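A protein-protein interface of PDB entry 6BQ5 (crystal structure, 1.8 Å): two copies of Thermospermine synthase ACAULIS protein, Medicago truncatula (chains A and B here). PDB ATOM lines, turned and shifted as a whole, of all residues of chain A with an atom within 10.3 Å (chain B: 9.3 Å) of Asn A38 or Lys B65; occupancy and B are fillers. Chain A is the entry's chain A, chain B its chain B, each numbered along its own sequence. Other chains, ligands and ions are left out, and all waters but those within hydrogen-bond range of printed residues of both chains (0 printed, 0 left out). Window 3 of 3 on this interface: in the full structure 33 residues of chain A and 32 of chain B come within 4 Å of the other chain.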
ATOM      1  N   GLU A  32      30.062 -11.511 -15.342  1.00  0.00           N
ATOM      2  CA  GLU A  32      30.160 -10.087 -15.455  1.00  0.00           C
ATOM      3  C   GLU A  32      31.591  -9.658 -15.248  1.00  0.00           C
ATOM      4  O   GLU A  32      32.281 -10.144 -14.358  1.00  0.00           O
ATOM      5  CB  GLU A  32      29.194  -9.370 -14.520  1.00  0.00           C
ATOM      6  CG  GLU A  32      29.654  -9.138 -13.105  1.00  0.00           C
ATOM      7  CD  GLU A  32      28.732  -8.119 -12.394  1.00  0.00           C
ATOM      8  OE1 GLU A  32      29.264  -7.246 -11.655  1.00  0.00           O
ATOM      9  OE2 GLU A  32      27.479  -8.177 -12.622  1.00  0.00           O
ATOM     10  N   GLU A  33      32.078  -8.789 -16.125  1.00  0.00           N
ATOM     11  CA  GLU A  33      33.400  -8.270 -15.922  1.00  0.00           C
ATOM     12  C   GLU A  33      33.366  -6.764 -16.092  1.00  0.00           C
ATOM     13  O   GLU A  33      32.744  -6.264 -17.009  1.00  0.00           O
ATOM     14  CB  GLU A  33      34.393  -8.946 -16.861  1.00  0.00           C
ATOM     15  CG  GLU A  33      35.775  -8.406 -16.594  1.00  0.00           C
ATOM     16  CD  GLU A  33      36.882  -9.040 -17.387  1.00  0.00           C
ATOM     17  OE1 GLU A  33      36.660 -10.107 -18.049  1.00  0.00           O
ATOM     18  OE2 GLU A  33      37.973  -8.454 -17.378  1.00  0.00           O
ATOM     19  N   GLU A  34      33.964  -6.036 -15.165  1.00  0.00           N
ATOM     20  CA  GLU A  34      34.056  -4.587 -15.327  1.00  0.00           C
ATOM     21  C   GLU A  34      35.283  -4.319 -16.223  1.00  0.00           C
ATOM     22  O   GLU A  34      36.405  -4.326 -15.767  1.00  0.00           O
ATOM     23  CB  GLU A  34      34.104  -3.851 -13.950  1.00  0.00           C
ATOM     24  CG  GLU A  34      33.893  -2.329 -14.074  1.00  0.00           C
ATOM     25  CD  GLU A  34      33.550  -1.558 -12.770  1.00  0.00           C
ATOM     26  OE1 GLU A  34      33.202  -2.210 -11.753  1.00  0.00           O
ATOM     27  OE2 GLU A  34      33.622  -0.297 -12.781  1.00  0.00           O
ATOM     28  N   ILE A  35      35.070  -4.158 -17.526  1.00  0.00           N
ATOM     29  CA  ILE A  35      36.215  -4.097 -18.430  1.00  0.00           C
ATOM     30  C   ILE A  35      36.842  -2.697 -18.474  1.00  0.00           C
ATOM     31  O   ILE A  35      37.905  -2.512 -18.990  1.00  0.00           O
ATOM     32  CB  ILE A  35      35.927  -4.642 -19.850  1.00  0.00           C
ATOM     33  CG1 ILE A  35      34.827  -3.852 -20.537  1.00  0.00           C
ATOM     34  CG2 ILE A  35      35.560  -6.120 -19.795  1.00  0.00           C
ATOM     35  CD1 ILE A  35      34.675  -4.214 -22.002  1.00  0.00           C
ATOM     36  N   GLU A  36      36.189  -1.710 -17.916  1.00  0.00           N
ATOM     37  CA  GLU A  36      36.777  -0.395 -17.802  1.00  0.00           C
ATOM     38  C   GLU A  36      35.972   0.164 -16.665  1.00  0.00           C
ATOM     39  O   GLU A  36      34.932  -0.390 -16.322  1.00  0.00           O
ATOM     40  CB  GLU A  36      36.670   0.350 -19.166  1.00  0.00           C
ATOM     41  CG  GLU A  36      36.667   1.869 -19.165  1.00  0.00           C
ATOM     42  CD  GLU A  36      36.351   2.519 -20.555  1.00  0.00           C
ATOM     43  OE1 GLU A  36      36.547   1.837 -21.612  1.00  0.00           O
ATOM     44  OE2 GLU A  36      35.885   3.705 -20.582  1.00  0.00           O
ATOM     45  N   GLU A  37      36.472   1.208 -16.027  1.00  0.00           N
ATOM     46  CA  GLU A  37      35.774   1.769 -14.878  1.00  0.00           C
ATOM     47  C   GLU A  37      34.374   2.181 -15.352  1.00  0.00           C
ATOM     48  O   GLU A  37      34.222   2.817 -16.403  1.00  0.00           O
ATOM     49  CB  GLU A  37      36.536   2.984 -14.315  1.00  0.00           C
ATOM     50  CG  GLU A  37      36.528   3.020 -12.797  1.00  0.00           C
ATOM     51  CD  GLU A  37      36.950   4.393 -12.271  1.00  0.00           C
ATOM     52  OE1 GLU A  37      37.914   4.977 -12.828  1.00  0.00           O
ATOM     53  OE2 GLU A  37      36.308   4.892 -11.308  1.00  0.00           O
ATOM     54  N   ASN A  38      33.357   1.754 -14.623  1.00  0.00           N
ATOM     55  CA  ASN A  38      31.979   2.147 -14.924  1.00  0.00           C
ATOM     56  C   ASN A  38      31.392   1.467 -16.171  1.00  0.00           C
ATOM     57  O   ASN A  38      30.331   1.879 -16.654  1.00  0.00           O
ATOM     58  CB  ASN A  38      31.876   3.667 -15.055  1.00  0.00           C
ATOM     59  CG  ASN A  38      32.344   4.371 -13.806  1.00  0.00           C
ATOM     60  OD1 ASN A  38      33.072   5.337 -13.875  1.00  0.00           O
ATOM     61  ND2 ASN A  38      31.959   3.863 -12.686  1.00  0.00           N
ATOM     62  N   LEU A  39      32.038   0.412 -16.638  1.00  0.00           N
ATOM     63  CA  LEU A  39      31.605  -0.258 -17.835  1.00  0.00           C
ATOM     64  C   LEU A  39      31.605  -1.763 -17.585  1.00  0.00           C
ATOM     65  O   LEU A  39      32.660  -2.328 -17.370  1.00  0.00           O
ATOM     66  CB  LEU A  39      32.551   0.141 -18.976  1.00  0.00           C
ATOM     67  CG  LEU A  39      32.187  -0.392 -20.358  1.00  0.00           C
ATOM     68  CD1 LEU A  39      30.770   0.017 -20.766  1.00  0.00           C
ATOM     69  CD2 LEU A  39      33.221   0.062 -21.407  1.00  0.00           C
ATOM     70  N   ARG A  40      30.433  -2.408 -17.637  1.00  0.00           N
ATOM     71  CA  ARG A  40      30.314  -3.854 -17.403  1.00  0.00           C
ATOM     72  C   ARG A  40      29.913  -4.563 -18.648  1.00  0.00           C
ATOM     73  O   ARG A  40      29.019  -4.110 -19.347  1.00  0.00           O
ATOM     74  CB  ARG A  40      29.270  -4.130 -16.271  1.00  0.00           C
ATOM     75  CG  ARG A  40      29.920  -4.521 -14.964  1.00  0.00           C
ATOM     76  CD  ARG A  40      29.318  -3.987 -13.678  1.00  0.00           C
ATOM     77  NE  ARG A  40      27.938  -4.370 -13.472  1.00  0.00           N
ATOM     78  CZ  ARG A  40      27.270  -4.206 -12.310  1.00  0.00           C
ATOM     79  NH1 ARG A  40      27.903  -3.711 -11.222  1.00  0.00           N
ATOM     80  NH2 ARG A  40      26.008  -4.554 -12.226  1.00  0.00           N
ATOM     81  N   TRP A  41      30.580  -5.683 -18.915  1.00  0.00           N
ATOM     82  CA  TRP A  41      30.384  -6.532 -20.087  1.00  0.00           C
ATOM     83  C   TRP A  41      29.897  -7.868 -19.523  1.00  0.00           C
ATOM     84  O   TRP A  41      30.639  -8.521 -18.795  1.00  0.00           O
ATOM     85  CB  TRP A  41      31.762  -6.678 -20.742  1.00  0.00           C
ATOM     86  CG  TRP A  41      31.873  -7.250 -22.129  1.00  0.00           C
ATOM     87  CD1 TRP A  41      32.861  -8.075 -22.579  1.00  0.00           C
ATOM     88  CD2 TRP A  41      31.012  -7.013 -23.249  1.00  0.00           C
ATOM     89  NE1 TRP A  41      32.665  -8.379 -23.899  1.00  0.00           N
ATOM     90  CE2 TRP A  41      31.536  -7.741 -24.337  1.00  0.00           C
ATOM     91  CE3 TRP A  41      29.849  -6.268 -23.439  1.00  0.00           C
ATOM     92  CZ2 TRP A  41      30.935  -7.745 -25.590  1.00  0.00           C
ATOM     93  CZ3 TRP A  41      29.253  -6.274 -24.685  1.00  0.00           C
ATOM     94  CH2 TRP A  41      29.798  -7.007 -25.744  1.00  0.00           C
ATOM     95  N   CYS A  42      28.671  -8.289 -19.843  1.00  0.00           N
ATOM     96  CA  CYS A  42      28.150  -9.545 -19.237  1.00  0.00           C
ATOM     97  C   CYS A  42      27.763 -10.584 -20.281  1.00  0.00           C
ATOM     98  O   CYS A  42      27.160 -10.256 -21.303  1.00  0.00           O
ATOM     99  CB  CYS A  42      26.949  -9.230 -18.357  1.00  0.00           C
ATOM    100  SG  CYS A  42      27.237  -7.787 -17.303  1.00  0.00           S
ATOM    101  N   LYS B  27      28.708   3.615  -7.609  1.00  0.00           N
ATOM    102  CA  LYS B  27      28.614   2.336  -8.375  1.00  0.00           C
ATOM    103  C   LYS B  27      27.187   1.707  -8.390  1.00  0.00           C
ATOM    104  O   LYS B  27      27.024   0.521  -8.764  1.00  0.00           O
ATOM    105  CB  LYS B  27      29.657   1.336  -7.833  1.00  0.00           C
ATOM    106  CG  LYS B  27      29.624   1.136  -6.306  1.00  0.00           C
ATOM    107  CD  LYS B  27      30.765   0.265  -5.744  1.00  0.00           C
ATOM    108  CE  LYS B  27      32.182   0.851  -5.915  1.00  0.00           C
ATOM    109  NZ  LYS B  27      32.350   2.274  -5.480  1.00  0.00           N
ATOM    110  N   SER B  28      26.152   2.478  -8.044  1.00  0.00           N
ATOM    111  CA  SER B  28      24.845   1.873  -7.779  1.00  0.00           C
ATOM    112  C   SER B  28      23.848   1.901  -8.933  1.00  0.00           C
ATOM    113  O   SER B  28      23.004   0.995  -9.003  1.00  0.00           O
ATOM    114  CB  SER B  28      24.202   2.485  -6.521  1.00  0.00           C
ATOM    115  OG  SER B  28      23.602   3.738  -6.827  1.00  0.00           O
ATOM    116  N   CYS B  29      23.905   2.928  -9.793  1.00  0.00           N
ATOM    117  CA  CYS B  29      22.948   3.085 -10.903  1.00  0.00           C
ATOM    118  C   CYS B  29      23.608   2.805 -12.257  1.00  0.00           C
ATOM    119  O   CYS B  29      24.720   3.271 -12.524  1.00  0.00           O
ATOM    120  CB  CYS B  29      22.305   4.484 -10.936  1.00  0.00           C
ATOM    121  SG  CYS B  29      21.412   4.765  -9.376  1.00  0.00           S
ATOM    122  N   TRP B  30      22.897   2.015 -13.058  1.00  0.00           N
ATOM    123  CA  TRP B  30      23.405   1.461 -14.304  1.00  0.00           C
ATOM    124  C   TRP B  30      22.369   1.540 -15.386  1.00  0.00           C
ATOM    125  O   TRP B  30      21.167   1.347 -15.154  1.00  0.00           O
ATOM    126  CB  TRP B  30      23.815  -0.029 -14.121  1.00  0.00           C
ATOM    127  CG  TRP B  30      24.945  -0.209 -13.189  1.00  0.00           C
ATOM    128  CD1 TRP B  30      24.860  -0.298 -11.860  1.00  0.00           C
ATOM    129  CD2 TRP B  30      26.341  -0.241 -13.508  1.00  0.00           C
ATOM    130  NE1 TRP B  30      26.098  -0.378 -11.314  1.00  0.00           N
ATOM    131  CE2 TRP B  30      27.033  -0.391 -12.296  1.00  0.00           C
ATOM    132  CE3 TRP B  30      27.070  -0.205 -14.697  1.00  0.00           C
ATOM    133  CZ2 TRP B  30      28.423  -0.481 -12.219  1.00  0.00           C
ATOM    134  CZ3 TRP B  30      28.453  -0.276 -14.632  1.00  0.00           C
ATOM    135  CH2 TRP B  30      29.118  -0.437 -13.404  1.00  0.00           C
ATOM    136  N   TYR B  31      22.830   1.835 -16.573  1.00  0.00           N
ATOM    137  CA  TYR B  31      22.018   1.658 -17.749  1.00  0.00           C
ATOM    138  C   TYR B  31      22.461   0.323 -18.384  1.00  0.00           C
ATOM    139  O   TYR B  31      23.620   0.064 -18.493  1.00  0.00           O
ATOM    140  CB  TYR B  31      22.222   2.838 -18.709  1.00  0.00           C
ATOM    141  CG  TYR B  31      21.603   2.586 -20.091  1.00  0.00           C
ATOM    142  CD1 TYR B  31      20.238   2.627 -20.286  1.00  0.00           C
ATOM    143  CD2 TYR B  31      22.408   2.230 -21.176  1.00  0.00           C
ATOM    144  CE1 TYR B  31      19.677   2.382 -21.547  1.00  0.00           C
ATOM    145  CE2 TYR B  31      21.868   1.966 -22.445  1.00  0.00           C
ATOM    146  CZ  TYR B  31      20.499   2.035 -22.627  1.00  0.00           C
ATOM    147  OH  TYR B  31      19.964   1.776 -23.890  1.00  0.00           O
ATOM    148  N   TRP B  41      25.651  -5.000 -22.041  1.00  0.00           N
ATOM    149  CA  TRP B  41      26.582  -3.876 -22.038  1.00  0.00           C
ATOM    150  C   TRP B  41      26.010  -2.929 -20.990  1.00  0.00           C
ATOM    151  O   TRP B  41      24.866  -2.504 -21.119  1.00  0.00           O
ATOM    152  CB  TRP B  41      26.500  -3.252 -23.436  1.00  0.00           C
ATOM    153  CG  TRP B  41      27.555  -2.278 -23.873  1.00  0.00           C
ATOM    154  CD1 TRP B  41      27.342  -1.111 -24.544  1.00  0.00           C
ATOM    155  CD2 TRP B  41      28.975  -2.399 -23.729  1.00  0.00           C
ATOM    156  NE1 TRP B  41      28.533  -0.490 -24.811  1.00  0.00           N
ATOM    157  CE2 TRP B  41      29.553  -1.258 -24.319  1.00  0.00           C
ATOM    158  CE3 TRP B  41      29.813  -3.352 -23.148  1.00  0.00           C
ATOM    159  CZ2 TRP B  41      30.925  -1.046 -24.346  1.00  0.00           C
ATOM    160  CZ3 TRP B  41      31.175  -3.138 -23.175  1.00  0.00           C
ATOM    161  CH2 TRP B  41      31.718  -1.994 -23.769  1.00  0.00           C
ATOM    162  N   CYS B  42      26.785  -2.581 -19.963  1.00  0.00           N
ATOM    163  CA  CYS B  42      26.223  -1.746 -18.872  1.00  0.00           C
ATOM    164  C   CYS B  42      27.129  -0.543 -18.577  1.00  0.00           C
ATOM    165  O   CYS B  42      28.359  -0.675 -18.498  1.00  0.00           O
ATOM    166  CB  CYS B  42      26.002  -2.585 -17.639  1.00  0.00           C
ATOM    167  SG  CYS B  42      25.210  -4.178 -17.959  1.00  0.00           S
ATOM    168  N   PHE B  43      26.513   0.643 -18.521  1.00  0.00           N
ATOM    169  CA  PHE B  43      27.213   1.896 -18.277  1.00  0.00           C
ATOM    170  C   PHE B  43      26.726   2.434 -16.915  1.00  0.00           C
ATOM    171  O   PHE B  43      25.521   2.527 -16.669  1.00  0.00           O
ATOM    172  CB  PHE B  43      26.832   3.002 -19.276  1.00  0.00           C
ATOM    173  CG  PHE B  43      26.927   2.647 -20.716  1.00  0.00           C
ATOM    174  CD1 PHE B  43      27.741   1.633 -21.187  1.00  0.00           C
ATOM    175  CD2 PHE B  43      26.232   3.419 -21.633  1.00  0.00           C
ATOM    176  CE1 PHE B  43      27.813   1.386 -22.533  1.00  0.00           C
ATOM    177  CE2 PHE B  43      26.319   3.191 -22.976  1.00  0.00           C
ATOM    178  CZ  PHE B  43      27.102   2.161 -23.435  1.00  0.00           C
ATOM    179  N   ALA B  44      27.651   2.882 -16.084  1.00  0.00           N
ATOM    180  CA  ALA B  44      27.253   3.527 -14.808  1.00  0.00           C
ATOM    181  C   ALA B  44      26.569   4.847 -15.146  1.00  0.00           C
ATOM    182  O   ALA B  44      27.001   5.569 -16.050  1.00  0.00           O
ATOM    183  CB  ALA B  44      28.450   3.720 -13.887  1.00  0.00           C
ATOM    184  N   LEU B  45      25.524   5.175 -14.395  1.00  0.00           N
ATOM    185  CA  LEU B  45      24.657   6.323 -14.686  1.00  0.00           C
ATOM    186  C   LEU B  45      24.905   7.424 -13.637  1.00  0.00           C
ATOM    187  O   LEU B  45      24.927   7.136 -12.465  1.00  0.00           O
ATOM    188  CB  LEU B  45      23.202   5.932 -14.547  1.00  0.00           C
ATOM    189  CG  LEU B  45      22.328   5.587 -15.696  1.00  0.00           C
ATOM    190  CD1 LEU B  45      20.952   5.111 -15.194  1.00  0.00           C
ATOM    191  CD2 LEU B  45      22.128   6.796 -16.557  1.00  0.00           C
ATOM    192  N   ASN B  46      25.049   8.652 -14.095  1.00  0.00           N
ATOM    193  CA  ASN B  46      25.020   9.847 -13.233  1.00  0.00           C
ATOM    194  C   ASN B  46      23.623  10.273 -13.043  1.00  0.00           C
ATOM    195  O   ASN B  46      23.272  10.625 -11.961  1.00  0.00           O
ATOM    196  CB  ASN B  46      25.801  11.011 -13.867  1.00  0.00           C
ATOM    197  CG  ASN B  46      27.267  10.744 -13.905  1.00  0.00           C
ATOM    198  OD1 ASN B  46      27.829  10.236 -12.925  1.00  0.00           O
ATOM    199  ND2 ASN B  46      27.893  11.019 -15.018  1.00  0.00           N
ATOM    200  N   SER B  47      22.840  10.317 -14.119  1.00  0.00           N
ATOM    201  CA  SER B  47      21.460  10.763 -14.068  1.00  0.00           C
ATOM    202  C   SER B  47      20.705  10.452 -15.321  1.00  0.00           C
ATOM    203  O   SER B  47      21.278  10.059 -16.340  1.00  0.00           O
ATOM    204  CB  SER B  47      21.336  12.274 -13.745  1.00  0.00           C
ATOM    205  OG  SER B  47      21.680  13.081 -14.838  1.00  0.00           O
ATOM    206  N   LEU B  62      20.465  10.271 -21.145  1.00  0.00           N
ATOM    207  CA  LEU B  62      21.105   9.743 -19.964  1.00  0.00           C
ATOM    208  C   LEU B  62      22.423  10.436 -19.818  1.00  0.00           C
ATOM    209  O   LEU B  62      23.041  10.815 -20.816  1.00  0.00           O
ATOM    210  CB  LEU B  62      21.363   8.260 -20.108  1.00  0.00           C
ATOM    211  CG  LEU B  62      20.150   7.398 -20.485  1.00  0.00           C
ATOM    212  CD1 LEU B  62      20.567   5.942 -20.580  1.00  0.00           C
ATOM    213  CD2 LEU B  62      19.020   7.541 -19.508  1.00  0.00           C
ATOM    214  N   ASP B  63      22.850  10.641 -18.589  1.00  0.00           N
ATOM    215  CA  ASP B  63      24.149  11.171 -18.372  1.00  0.00           C
ATOM    216  C   ASP B  63      24.912   9.983 -17.786  1.00  0.00           C
ATOM    217  O   ASP B  63      24.662   9.570 -16.672  1.00  0.00           O
ATOM    218  CB  ASP B  63      24.088  12.407 -17.489  1.00  0.00           C
ATOM    219  CG  ASP B  63      25.462  12.950 -17.130  1.00  0.00           C
ATOM    220  OD1 ASP B  63      26.458  12.431 -17.630  1.00  0.00           O
ATOM    221  OD2 ASP B  63      25.547  13.879 -16.311  1.00  0.00           O
ATOM    222  N   THR B  64      25.796   9.436 -18.587  1.00  0.00           N
ATOM    223  CA  THR B  64      26.511   8.189 -18.287  1.00  0.00           C
ATOM    224  C   THR B  64      27.922   8.504 -17.951  1.00  0.00           C
ATOM    225  O   THR B  64      28.477   9.450 -18.458  1.00  0.00           O
ATOM    226  CB  THR B  64      26.501   7.156 -19.448  1.00  0.00           C
ATOM    227  OG1 THR B  64      27.494   7.458 -20.433  1.00  0.00           O
ATOM    228  CG2 THR B  64      25.193   7.062 -20.115  1.00  0.00           C
ATOM    229  N   LYS B  65      28.539   7.659 -17.150  1.00  0.00           N
ATOM    230  CA  LYS B  65      29.933   7.890 -16.753  1.00  0.00           C
ATOM    231  C   LYS B  65      30.928   7.582 -17.839  1.00  0.00           C
ATOM    232  O   LYS B  65      31.729   8.457 -18.177  1.00  0.00           O
ATOM    233  CB  LYS B  65      30.285   7.128 -15.502  1.00  0.00           C
ATOM    234  CG  LYS B  65      29.553   7.671 -14.293  1.00  0.00           C
ATOM    235  CD  LYS B  65      30.461   7.672 -13.067  1.00  0.00           C
ATOM    236  CE  LYS B  65      29.779   7.011 -11.911  1.00  0.00           C
ATOM    237  NZ  LYS B  65      28.770   7.936 -11.352  1.00  0.00           N
ATOM    238  N   PRO B  66      30.882   6.368 -18.419  1.00  0.00           N
ATOM    239  CA  PRO B  66      31.927   6.095 -19.440  1.00  0.00           C
ATOM    240  C   PRO B  66      31.766   6.908 -20.777  1.00  0.00           C
ATOM    241  O   PRO B  66      32.742   7.255 -21.405  1.00  0.00           O
ATOM    242  CB  PRO B  66      31.786   4.603 -19.692  1.00  0.00           C
ATOM    243  CG  PRO B  66      30.398   4.283 -19.282  1.00  0.00           C
ATOM    244  CD  PRO B  66      29.965   5.234 -18.215  1.00  0.00           C
ATOM    245  N   PHE B  67      30.559   7.228 -21.190  1.00  0.00           N
ATOM    246  CA  PHE B  67      30.349   7.759 -22.540  1.00  0.00           C
ATOM    247  C   PHE B  67      29.699   9.125 -22.573  1.00  0.00           C
ATOM    248  O   PHE B  67      29.422   9.588 -23.649  1.00  0.00           O
ATOM    249  CB  PHE B  67      29.579   6.714 -23.383  1.00  0.00           C
ATOM    250  CG  PHE B  67      30.328   5.411 -23.532  1.00  0.00           C
ATOM    251  CD1 PHE B  67      31.588   5.392 -24.084  1.00  0.00           C
ATOM    252  CD2 PHE B  67      29.780   4.234 -23.163  1.00  0.00           C
ATOM    253  CE1 PHE B  67      32.291   4.222 -24.240  1.00  0.00           C
ATOM    254  CE2 PHE B  67      30.469   3.049 -23.343  1.00  0.00           C
ATOM    255  CZ  PHE B  67      31.724   3.059 -23.850  1.00  0.00           C
ATOM    256  N   GLY B  68      29.528   9.774 -21.421  1.00  0.00           N
ATOM    257  CA  GLY B  68      28.911  11.085 -21.324  1.00  0.00           C
ATOM    258  C   GLY B  68      27.425  10.992 -21.577  1.00  0.00           C
ATOM    259  O   GLY B  68      26.793   9.927 -21.342  1.00  0.00           O
ATOM    260  N   LYS B  69      26.867  12.063 -22.108  1.00  0.00           N
ATOM    261  CA  LYS B  69      25.476  12.101 -22.466  1.00  0.00           C
ATOM    262  C   LYS B  69      25.159  11.182 -23.620  1.00  0.00           C
ATOM    263  O   LYS B  69      25.876  11.138 -24.613  1.00  0.00           O
ATOM    264  CB  LYS B  69      24.995  13.506 -22.722  1.00  0.00           C
ATOM    265  CG  LYS B  69      25.161  14.390 -21.485  1.00  0.00           C
ATOM    266  CD  LYS B  69      24.540  15.759 -21.738  1.00  0.00           C
ATOM    267  CE  LYS B  69      25.567  16.859 -21.839  1.00  0.00           C
ATOM    268  NZ  LYS B  69      25.714  17.475 -20.464  1.00  0.00           N
ATOM    269  N   ALA B  70      24.084  10.433 -23.453  1.00  0.00           N
ATOM    270  CA  ALA B  70      23.667   9.367 -24.359  1.00  0.00           C
ATOM    271  C   ALA B  70      22.206   9.464 -24.691  1.00  0.00           C
ATOM    272  O   ALA B  70      21.330   9.431 -23.785  1.00  0.00           O
ATOM    273  CB  ALA B  70      23.921   8.035 -23.704  1.00  0.00           C
ATOM    274  N   ALA B  80      26.303   8.607 -28.222  1.00  0.00           N
ATOM    275  CA  ALA B  80      26.979   8.904 -26.985  1.00  0.00           C
ATOM    276  C   ALA B  80      27.929  10.058 -27.195  1.00  0.00           C
ATOM    277  O   ALA B  80      28.623  10.153 -28.203  1.00  0.00           O
ATOM    278  CB  ALA B  80      27.725   7.673 -26.519  1.00  0.00           C
ATOM    279  N   GLU B  81      27.976  10.958 -26.244  1.00  0.00           N
ATOM    280  CA  GLU B  81      28.783  12.139 -26.337  1.00  0.00           C
ATOM    281  C   GLU B  81      30.218  11.910 -26.743  1.00  0.00           C
ATOM    282  O   GLU B  81      30.748  12.626 -27.587  1.00  0.00           O
ATOM    283  CB  GLU B  81      28.743  12.843 -24.986  1.00  0.00           C
ATOM    284  CG  GLU B  81      29.433  14.181 -24.895  1.00  0.00           C
ATOM    285  CD  GLU B  81      29.379  14.748 -23.470  1.00  0.00           C
ATOM    286  OE1 GLU B  81      28.651  14.194 -22.594  1.00  0.00           O
ATOM    287  OE2 GLU B  81      30.033  15.756 -23.247  1.00  0.00           O
ATOM    288  N   THR B  82      30.881  10.950 -26.113  1.00  0.00           N
ATOM    289  CA  THR B  82      32.292  10.761 -26.340  1.00  0.00           C
ATOM    290  C   THR B  82      32.660  10.257 -27.723  1.00  0.00           C
ATOM    291  O   THR B  82      33.811  10.428 -28.138  1.00  0.00           O
ATOM    292  CB  THR B  82      32.935   9.781 -25.352  1.00  0.00           C
ATOM    293  OG1 THR B  82      32.181   8.558 -25.362  1.00  0.00           O
ATOM    294  CG2 THR B  82      32.938  10.369 -23.941  1.00  0.00           C
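The backbone carbonyl oxygen (O) of Asn A38 is in hydrogen-bond range of the backbone NH (N) of Ala B44, at 2.9 Å. The backbone carbonyl oxygen of Arg A40 lies within hydrogen-bond range of the backbone NH of Cys B42, 2.8 Å away.
NE of Arg A40 lies within salt-bridge range of OE1 of Glu A32 (3.7 Å). N of Trp A41 sits at hydrogen-bond distance from O of Glu A33 (2.9 Å). OE2 of Glu A34 lies within hydrogen-bond range of N of Asn A38 (2.8 Å). The indole nitrogen (NE1) of Trp B30 lies within hydrogen-bond range of the backbone carbonyl oxygen (O) of Lys B27, at 2.9 Å. The backbone NH (N) of Tyr B31 is in hydrogen-bond range of the backbone carbonyl oxygen (O) of Phe B43. O of Phe B67 is in hydrogen-bond range of N of Thr B82 (3.2 Å).
Asn A38 touches Trp B30 (O to CZ3, 3.5 Å). Asn A38 touches Phe B43. Asn A38 touches Lys B65. Pro B66 touches Asn A38 (CG to O, 3.6 Å). CH2 of Trp B41 touches CD2 of Leu A39 (3.5 Å). Leu A39 touches Cys B42 (CA to O, 3.3 Å). Phe B43 touches Leu A39 (CD1 to CD1, 3.5 Å). Trp B30 touches Arg A40. O of Arg A40 touches C of Trp B41 (3.6 Å). Trp A41 touches Trp B41 (CE3 to CE3, 2.9 Å).
Glu A32 touches none of the printed residues of chain B. Glu A37 touches none of the printed residues of chain B. Of chain B, only Trp B30 (3.5 Å), Cys B42 (3.7 Å), Phe B43 (3.5 Å), Ala B44 (2.9 Å), Lys B65 (3.6 Å) and Pro B66 (3.6 Å) come within 4 Å of Asn A38. Of the printed residues of chain B, Leu A39 touches Trp B41, Cys B42, Phe B43 and Phe B67. Of the printed residues of chain B, Trp A41 touches Trp B41. Ser B28 touches none of the printed residues of chain A. Of the printed residues of chain A, Ala B44 touches Asn A38. No residue of chain A comes within 4 Å of Asn B46. No residue of chain A comes within 4 Å of Thr B64. Lys B65 touches one residue of chain A. Of chain A, only Asn A38 (3.6 Å) comes within 4 Å of Pro B66. Gly B68 touches none of the printed residues of chain A. The nearest residue of chain A that does not touch Lys B65 is Glu A37 (5.9 Å).
Hydrophobic or aromatic side chains of chain B within 4 Å of the printed part of chain A: Trp B30, Trp B41, Phe B43, Ala B44, Pro B66 and Phe B67. Hydrophobic or aromatic side chains of chain A within 4 Å of the printed part of chain B: Ile A35, Leu A39 and Trp A41. Among the printed residues, no Asp or Glu carboxylate lies within 4 Å of a Lys or Arg side-chain nitrogen of the other chain.
Trp A41 touches its own counterpart, Trp B41.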
